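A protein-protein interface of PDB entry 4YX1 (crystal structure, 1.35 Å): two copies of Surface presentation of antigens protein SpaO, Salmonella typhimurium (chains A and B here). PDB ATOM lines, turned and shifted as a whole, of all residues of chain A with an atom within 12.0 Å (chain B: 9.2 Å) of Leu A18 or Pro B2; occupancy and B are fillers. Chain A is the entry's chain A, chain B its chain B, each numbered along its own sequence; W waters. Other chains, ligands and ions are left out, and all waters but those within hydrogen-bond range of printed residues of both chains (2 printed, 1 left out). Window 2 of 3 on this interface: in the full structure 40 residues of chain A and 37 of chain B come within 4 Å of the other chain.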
ATOM      1  N   LYS A  14     -20.000  26.869  24.285  1.00  0.00           N
ATOM      2  CA  LYS A  14     -21.192  26.074  24.098  1.00  0.00           C
ATOM      3  C   LYS A  14     -20.878  24.905  23.192  1.00  0.00           C
ATOM      4  O   LYS A  14     -20.086  25.037  22.260  1.00  0.00           O
ATOM      5  CB  LYS A  14     -22.308  26.928  23.492  1.00  0.00           C
ATOM      6  CG  LYS A  14     -23.663  26.252  23.406  1.00  0.00           C
ATOM      7  CD  LYS A  14     -24.391  26.296  24.738  1.00  0.00           C
ATOM      8  CE  LYS A  14     -25.761  25.654  24.629  1.00  0.00           C
ATOM      9  NZ  LYS A  14     -26.252  25.193  25.954  1.00  0.00           N
ATOM     10  N   ASN A  15     -21.499  23.765  23.463  1.00  0.00           N
ATOM     11  CA  ASN A  15     -21.500  22.661  22.518  1.00  0.00           C
ATOM     12  C   ASN A  15     -22.547  22.925  21.465  1.00  0.00           C
ATOM     13  O   ASN A  15     -23.725  23.077  21.788  1.00  0.00           O
ATOM     14  CB  ASN A  15     -21.783  21.338  23.226  1.00  0.00           C
ATOM     15  CG  ASN A  15     -20.733  21.000  24.250  1.00  0.00           C
ATOM     16  OD1 ASN A  15     -19.560  20.895  23.932  1.00  0.00           O
ATOM     17  ND2 ASN A  15     -21.149  20.828  25.488  1.00  0.00           N
ATOM     18  N   VAL A  16     -22.124  23.006  20.213  1.00  0.00           N
ATOM     19  CA  VAL A  16     -23.043  23.341  19.134  1.00  0.00           C
ATOM     20  C   VAL A  16     -22.965  22.309  18.015  1.00  0.00           C
ATOM     21  O   VAL A  16     -21.975  21.598  17.874  1.00  0.00           O
ATOM     22  CB  VAL A  16     -22.765  24.756  18.567  1.00  0.00           C
ATOM     23  CG1 VAL A  16     -22.885  25.799  19.661  1.00  0.00           C
ATOM     24  CG2 VAL A  16     -21.400  24.822  17.885  1.00  0.00           C
ATOM     25  N   THR A  17     -24.022  22.211  17.223  1.00  0.00           N
ATOM     26  CA  THR A  17     -23.989  21.288  16.103  1.00  0.00           C
ATOM     27  C   THR A  17     -23.252  21.925  14.929  1.00  0.00           C
ATOM     28  O   THR A  17     -23.083  23.150  14.866  1.00  0.00           O
ATOM     29  CB  THR A  17     -25.393  20.900  15.644  1.00  0.00           C
ATOM     30  OG1 THR A  17     -26.009  22.044  15.044  1.00  0.00           O
ATOM     31  CG2 THR A  17     -26.230  20.443  16.825  1.00  0.00           C
ATOM     32  N   LEU A  18     -22.846  21.097  13.976  1.00  0.00           N
ATOM     33  CA  LEU A  18     -22.241  21.617  12.757  1.00  0.00           C
ATOM     34  C   LEU A  18     -23.202  22.565  12.023  1.00  0.00           C
ATOM     35  O   LEU A  18     -22.788  23.605  11.541  1.00  0.00           O
ATOM     36  CB  LEU A  18     -21.807  20.471  11.841  1.00  0.00           C
ATOM     37  CG  LEU A  18     -20.724  19.537  12.389  1.00  0.00           C
ATOM     38  CD1 LEU A  18     -20.424  18.465  11.369  1.00  0.00           C
ATOM     39  CD2 LEU A  18     -19.457  20.295  12.747  1.00  0.00           C
ATOM     40  N   ALA A  19     -24.483  22.214  11.969  1.00  0.00           N
ATOM     41  CA  ALA A  19     -25.475  23.074  11.323  1.00  0.00           C
ATOM     42  C   ALA A  19     -25.572  24.436  12.013  1.00  0.00           C
ATOM     43  O   ALA A  19     -25.667  25.473  11.364  1.00  0.00           O
ATOM     44  CB  ALA A  19     -26.835  22.393  11.305  1.00  0.00           C
ATOM     45  N   GLU A  20     -25.546  24.438  13.336  1.00  0.00           N
ATOM     46  CA  GLU A  20     -25.582  25.698  14.073  1.00  0.00           C
ATOM     47  C   GLU A  20     -24.335  26.529  13.777  1.00  0.00           C
ATOM     48  O   GLU A  20     -24.418  27.746  13.587  1.00  0.00           O
ATOM     49  CB  GLU A  20     -25.714  25.433  15.573  1.00  0.00           C
ATOM     50  CG  GLU A  20     -27.106  24.946  15.975  1.00  0.00           C
ATOM     51  CD  GLU A  20     -27.188  24.410  17.395  1.00  0.00           C
ATOM     52  OE1 GLU A  20     -26.142  24.066  17.982  1.00  0.00           O
ATOM     53  OE2 GLU A  20     -28.320  24.323  17.920  1.00  0.00           O
ATOM     54  N   LEU A  21     -23.183  25.875  13.694  1.00  0.00           N
ATOM     55  CA  LEU A  21     -21.952  26.595  13.409  1.00  0.00           C
ATOM     56  C   LEU A  21     -21.977  27.177  11.997  1.00  0.00           C
ATOM     57  O   LEU A  21     -21.561  28.318  11.788  1.00  0.00           O
ATOM     58  CB  LEU A  21     -20.748  25.680  13.593  1.00  0.00           C
ATOM     59  CG  LEU A  21     -19.455  26.408  13.936  1.00  0.00           C
ATOM     60  CD1 LEU A  21     -19.546  27.091  15.285  1.00  0.00           C
ATOM     61  CD2 LEU A  21     -18.326  25.427  13.942  1.00  0.00           C
ATOM     62  N   GLU A  22     -22.497  26.401  11.042  1.00  0.00           N
ATOM     63  CA  GLU A  22     -22.689  26.860   9.666  1.00  0.00           C
ATOM     64  C   GLU A  22     -23.533  28.134   9.630  1.00  0.00           C
ATOM     65  O   GLU A  22     -23.192  29.115   8.957  1.00  0.00           O
ATOM     66  CB  GLU A  22     -23.360  25.766   8.828  1.00  0.00           C
ATOM     67  CG  GLU A  22     -22.441  24.959   7.932  1.00  0.00           C
ATOM     68  CD  GLU A  22     -22.189  25.642   6.587  1.00  0.00           C
ATOM     69  OE1 GLU A  22     -22.959  25.402   5.622  1.00  0.00           O
ATOM     70  OE2 GLU A  22     -21.216  26.426   6.499  1.00  0.00           O
ATOM     71  N   ALA A  23     -24.636  28.120  10.365  1.00  0.00           N
ATOM     72  CA  ALA A  23     -25.539  29.267  10.397  1.00  0.00           C
ATOM     73  C   ALA A  23     -24.840  30.485  10.987  1.00  0.00           C
ATOM     74  O   ALA A  23     -25.021  31.606  10.510  1.00  0.00           O
ATOM     75  CB  ALA A  23     -26.799  28.928  11.191  1.00  0.00           C
ATOM     76  N   MET A  24     -24.030  30.264  12.020  1.00  0.00           N
ATOM     77  CA  MET A  24     -23.258  31.346  12.609  1.00  0.00           C
ATOM     78  C   MET A  24     -22.308  31.973  11.595  1.00  0.00           C
ATOM     79  O   MET A  24     -22.132  33.194  11.555  1.00  0.00           O
ATOM     80  CB  MET A  24     -22.476  30.825  13.807  1.00  0.00           C
ATOM     81  CG  MET A  24     -21.261  31.657  14.189  1.00  0.00           C
ATOM     82  SD  MET A  24     -20.378  30.813  15.685  1.00  0.00           S
ATOM     83  CE  MET A  24     -22.109  30.222  16.485  1.00  0.00           C
ATOM     84  N   GLY A  25     -21.698  31.124  10.772  1.00  0.00           N
ATOM     85  CA  GLY A  25     -20.733  31.573   9.783  1.00  0.00           C
ATOM     86  C   GLY A  25     -21.326  32.465   8.706  1.00  0.00           C
ATOM     87  O   GLY A  25     -20.585  33.129   7.995  1.00  0.00           O
ATOM     88  N   GLN A  26     -22.653  32.487   8.594  1.00  0.00           N
ATOM     89  CA  GLN A  26     -23.344  33.378   7.661  1.00  0.00           C
ATOM     90  C   GLN A  26     -23.565  34.776   8.220  1.00  0.00           C
ATOM     91  O   GLN A  26     -24.004  35.664   7.498  1.00  0.00           O
ATOM     92  CB  GLN A  26     -24.695  32.781   7.263  1.00  0.00           C
ATOM     93  CG  GLN A  26     -24.582  31.487   6.504  1.00  0.00           C
ATOM     94  CD  GLN A  26     -23.871  31.668   5.187  1.00  0.00           C
ATOM     95  OE1 GLN A  26     -22.781  31.141   4.978  1.00  0.00           O
ATOM     96  NE2 GLN A  26     -24.488  32.411   4.283  1.00  0.00           N
ATOM     97  N   GLN A  27     -23.252  34.980   9.496  1.00  0.00           N
ATOM     98  CA  GLN A  27     -23.542  36.245  10.156  1.00  0.00           C
ATOM     99  C   GLN A  27     -22.329  37.151  10.239  1.00  0.00           C
ATOM    100  O   GLN A  27     -21.183  36.695  10.259  1.00  0.00           O
ATOM    101  CB  GLN A  27     -24.093  35.985  11.558  1.00  0.00           C
ATOM    102  CG  GLN A  27     -25.355  35.138  11.560  1.00  0.00           C
ATOM    103  CD  GLN A  27     -26.525  35.849  10.901  1.00  0.00           C
ATOM    104  OE1 GLN A  27     -27.265  36.600  11.546  1.00  0.00           O
ATOM    105  NE2 GLN A  27     -26.689  35.627   9.603  1.00  0.00           N
ATOM    106  N   LEU A  30     -22.727  38.669  15.779  1.00  0.00           N
ATOM    107  CA  LEU A  30     -23.259  37.562  16.565  1.00  0.00           C
ATOM    108  C   LEU A  30     -23.673  38.047  17.943  1.00  0.00           C
ATOM    109  O   LEU A  30     -22.882  38.663  18.650  1.00  0.00           O
ATOM    110  CB  LEU A  30     -22.227  36.440  16.691  1.00  0.00           C
ATOM    111  CG  LEU A  30     -21.934  35.600  15.446  1.00  0.00           C
ATOM    112  CD1 LEU A  30     -23.194  34.943  14.930  1.00  0.00           C
ATOM    113  CD2 LEU A  30     -21.276  36.382  14.342  1.00  0.00           C
ATOM    114  N   PRO B   2     -23.631  14.088  13.355  1.00  0.00           N
ATOM    115  CA  PRO B   2     -22.315  14.284  13.975  1.00  0.00           C
ATOM    116  C   PRO B   2     -22.407  14.677  15.447  1.00  0.00           C
ATOM    117  O   PRO B   2     -23.449  15.137  15.905  1.00  0.00           O
ATOM    118  CB  PRO B   2     -21.702  15.417  13.141  1.00  0.00           C
ATOM    119  CG  PRO B   2     -22.869  16.114  12.528  1.00  0.00           C
ATOM    120  CD  PRO B   2     -23.873  15.041  12.258  1.00  0.00           C
ATOM    121  N   VAL B   3     -21.318  14.468  16.174  1.00  0.00           N
ATOM    122  CA  VAL B   3     -21.188  14.917  17.556  1.00  0.00           C
ATOM    123  C   VAL B   3     -21.140  16.443  17.572  1.00  0.00           C
ATOM    124  O   VAL B   3     -20.769  17.071  16.581  1.00  0.00           O
ATOM    125  CB  VAL B   3     -19.912  14.309  18.219  1.00  0.00           C
ATOM    126  CG1 VAL B   3     -19.617  14.912  19.587  1.00  0.00           C
ATOM    127  CG2 VAL B   3     -20.046  12.797  18.329  1.00  0.00           C
ATOM    128  N   ASP B   4     -21.533  17.045  18.683  1.00  0.00           N
ATOM    129  CA  ASP B   4     -21.367  18.479  18.856  1.00  0.00           C
ATOM    130  C   ASP B   4     -19.902  18.895  18.838  1.00  0.00           C
ATOM    131  O   ASP B   4     -19.006  18.125  19.182  1.00  0.00           O
ATOM    132  CB  ASP B   4     -21.981  18.935  20.178  1.00  0.00           C
ATOM    133  CG  ASP B   4     -23.482  18.746  20.229  1.00  0.00           C
ATOM    134  OD1 ASP B   4     -24.125  18.539  19.171  1.00  0.00           O
ATOM    135  OD2 ASP B   4     -24.031  18.842  21.348  1.00  0.00           O
ATOM    136  N   VAL B   5     -19.664  20.131  18.442  1.00  0.00           N
ATOM    137  CA  VAL B   5     -18.340  20.720  18.530  1.00  0.00           C
ATOM    138  C   VAL B   5     -18.305  21.730  19.689  1.00  0.00           C
ATOM    139  O   VAL B   5     -19.326  22.316  20.058  1.00  0.00           O
ATOM    140  CB  VAL B   5     -17.934  21.400  17.194  1.00  0.00           C
ATOM    141  CG1 VAL B   5     -17.923  20.389  16.040  1.00  0.00           C
ATOM    142  CG2 VAL B   5     -18.850  22.541  16.878  1.00  0.00           C
ATOM    143  N   LYS B   6     -17.123  21.904  20.266  1.00  0.00           N
ATOM    144  CA  LYS B   6     -16.916  22.824  21.373  1.00  0.00           C
ATOM    145  C   LYS B   6     -16.559  24.222  20.862  1.00  0.00           C
ATOM    146  O   LYS B   6     -15.426  24.467  20.448  1.00  0.00           O
ATOM    147  CB  LYS B   6     -15.813  22.291  22.291  1.00  0.00           C
ATOM    148  CG  LYS B   6     -16.258  21.149  23.195  1.00  0.00           C
ATOM    149  CD  LYS B   6     -15.101  20.566  24.006  1.00  0.00           C
ATOM    150  CE  LYS B   6     -15.579  19.646  25.134  1.00  0.00           C
ATOM    151  NZ  LYS B   6     -15.784  20.377  26.423  1.00  0.00           N
ATOM    152  N   ALA B  44     -13.350  26.671  17.559  1.00  0.00           N
ATOM    153  CA  ALA B  44     -14.138  25.462  17.772  1.00  0.00           C
ATOM    154  C   ALA B  44     -13.246  24.250  17.637  1.00  0.00           C
ATOM    155  O   ALA B  44     -12.503  24.136  16.673  1.00  0.00           O
ATOM    156  CB  ALA B  44     -15.291  25.374  16.798  1.00  0.00           C
ATOM    157  N   ASN B  45     -13.312  23.359  18.619  1.00  0.00           N
ATOM    158  CA  ASN B  45     -12.472  22.170  18.619  1.00  0.00           C
ATOM    159  C   ASN B  45     -11.008  22.504  18.362  1.00  0.00           C
ATOM    160  O   ASN B  45     -10.316  21.777  17.645  1.00  0.00           O
ATOM    161  CB  ASN B  45     -12.957  21.154  17.571  1.00  0.00           C
ATOM    162  CG  ASN B  45     -14.163  20.370  18.038  1.00  0.00           C
ATOM    163  OD1 ASN B  45     -14.738  20.666  19.089  1.00  0.00           O
ATOM    164  ND2 ASN B  45     -14.566  19.369  17.256  1.00  0.00           N
ATOM    165  N   LEU B  49     -11.634  29.958  13.977  1.00  0.00           N
ATOM    166  CA  LEU B  49     -12.652  30.177  12.956  1.00  0.00           C
ATOM    167  C   LEU B  49     -12.702  31.601  12.444  1.00  0.00           C
ATOM    168  O   LEU B  49     -13.098  31.841  11.309  1.00  0.00           O
ATOM    169  CB  LEU B  49     -14.034  29.820  13.492  1.00  0.00           C
ATOM    170  CG  LEU B  49     -14.163  28.433  14.125  1.00  0.00           C
ATOM    171  CD1 LEU B  49     -15.604  28.204  14.572  1.00  0.00           C
ATOM    172  CD2 LEU B  49     -13.693  27.340  13.169  1.00  0.00           C
HETATM  173  O   HOH W   1     -25.763  20.649  21.823  1.00  0.00           O
HETATM  174  O   HOH W   2     -23.050  18.330  14.849  1.00  0.00           O
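Of the printed residues of chain B, Lys A14 touches Val B5 (3.6 Å) and Lys B6 (3.9 Å).
Of the printed residues of chain B, Asn A15 touches Asp B4, Val B5 and Lys B6.
Of the printed residues of chain B, Val A16 touches Asp B4 and Val B5.
Thr A17 touches just one residue of chain B: Asp B4 (3.7 Å).
Leu A18 touches just these residues of chain B: Pro B2 and Val B5.
No residue of chain B comes within 4 Å of Ala A19.
Pro B2 touches just one residue of chain A: Leu A18 (3.6 Å).
Val B3 touches none of the printed residues of chain A.
Of chain A, only Lys A14, Asn A15, Val A16 and Leu A18 come within 4 Å of Val B5.
Printed residues of chain A within 4 Å of Lys B6: Lys A14 and Asn A15.
The nearest residue of chain A that does not touch Pro B2 is Thr A17 (6.1 Å).
The nearest printed residue of chain B that does not touch Lys A14 is Asp B4 (6.7 Å).
No position is printed for both chains.
Of the 11 pairs that touch across the chains among the printed residues, none has its exchanged pair printed and touching as well.
Among the printed residues, pairs that only touch across the chains: Lys A14 with Val B5 (3.6 Å), Lys A14 with Lys B6 (3.9 Å), Asn A15 with Asp B4 (3.8 Å), Asn A15 with Val B5 (3.3 Å), Asn A15 with Lys B6 (3.4 Å), Val A16 with Asp B4 (3.3 Å), Thr A17 with Asp B4 (3.7 Å), Leu A18 with Pro B2 (3.6 Å), Leu A18 with Val B5 (3.6 Å) and Leu A21 with Leu B49 (3.9 Å).
The backbone NH of Ala A19 lies close to the side-chain hydroxyl of Thr A17 (3.4 Å).
N of Thr A17 lies within hydrogen-bond range of OE1 of Glu A20.
N of Lys B6 sits at hydrogen-bond distance from OD1 of Asn B45 (2.9 Å).
Printed residues of chain A that touch a printed residue of chain B: Lys A14, Asn A15, Val A16, Thr A17, Leu A18 and Leu A21.
Hydrophobic or aromatic side chains of chain A that line the printed part of chain B: Val A16, Leu A18 and Leu A21.
Hydrophobic or aromatic side chains of chain B within 4 Å of the printed part of chain A: Pro B2, Val B5 and Leu B49.
Along chain B the printed residues that touch a printed residue of chain A span positions 2 to 49.
Among the printed residues, 11 pairs touch across the chains.
N of Val B5 sits at hydrogen-bond distance from O of Val A16, 2.8 Å away.
Water W1 bridges OD2 of Asp B4 (2.5 Å) and O of Asn A15 (3.2 Å).
Water W2 lies within hydrogen-bond range of N of Leu A18 (2.9 Å), O of Val B3 (3.1 Å) and O of Pro B2 (3.4 Å).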
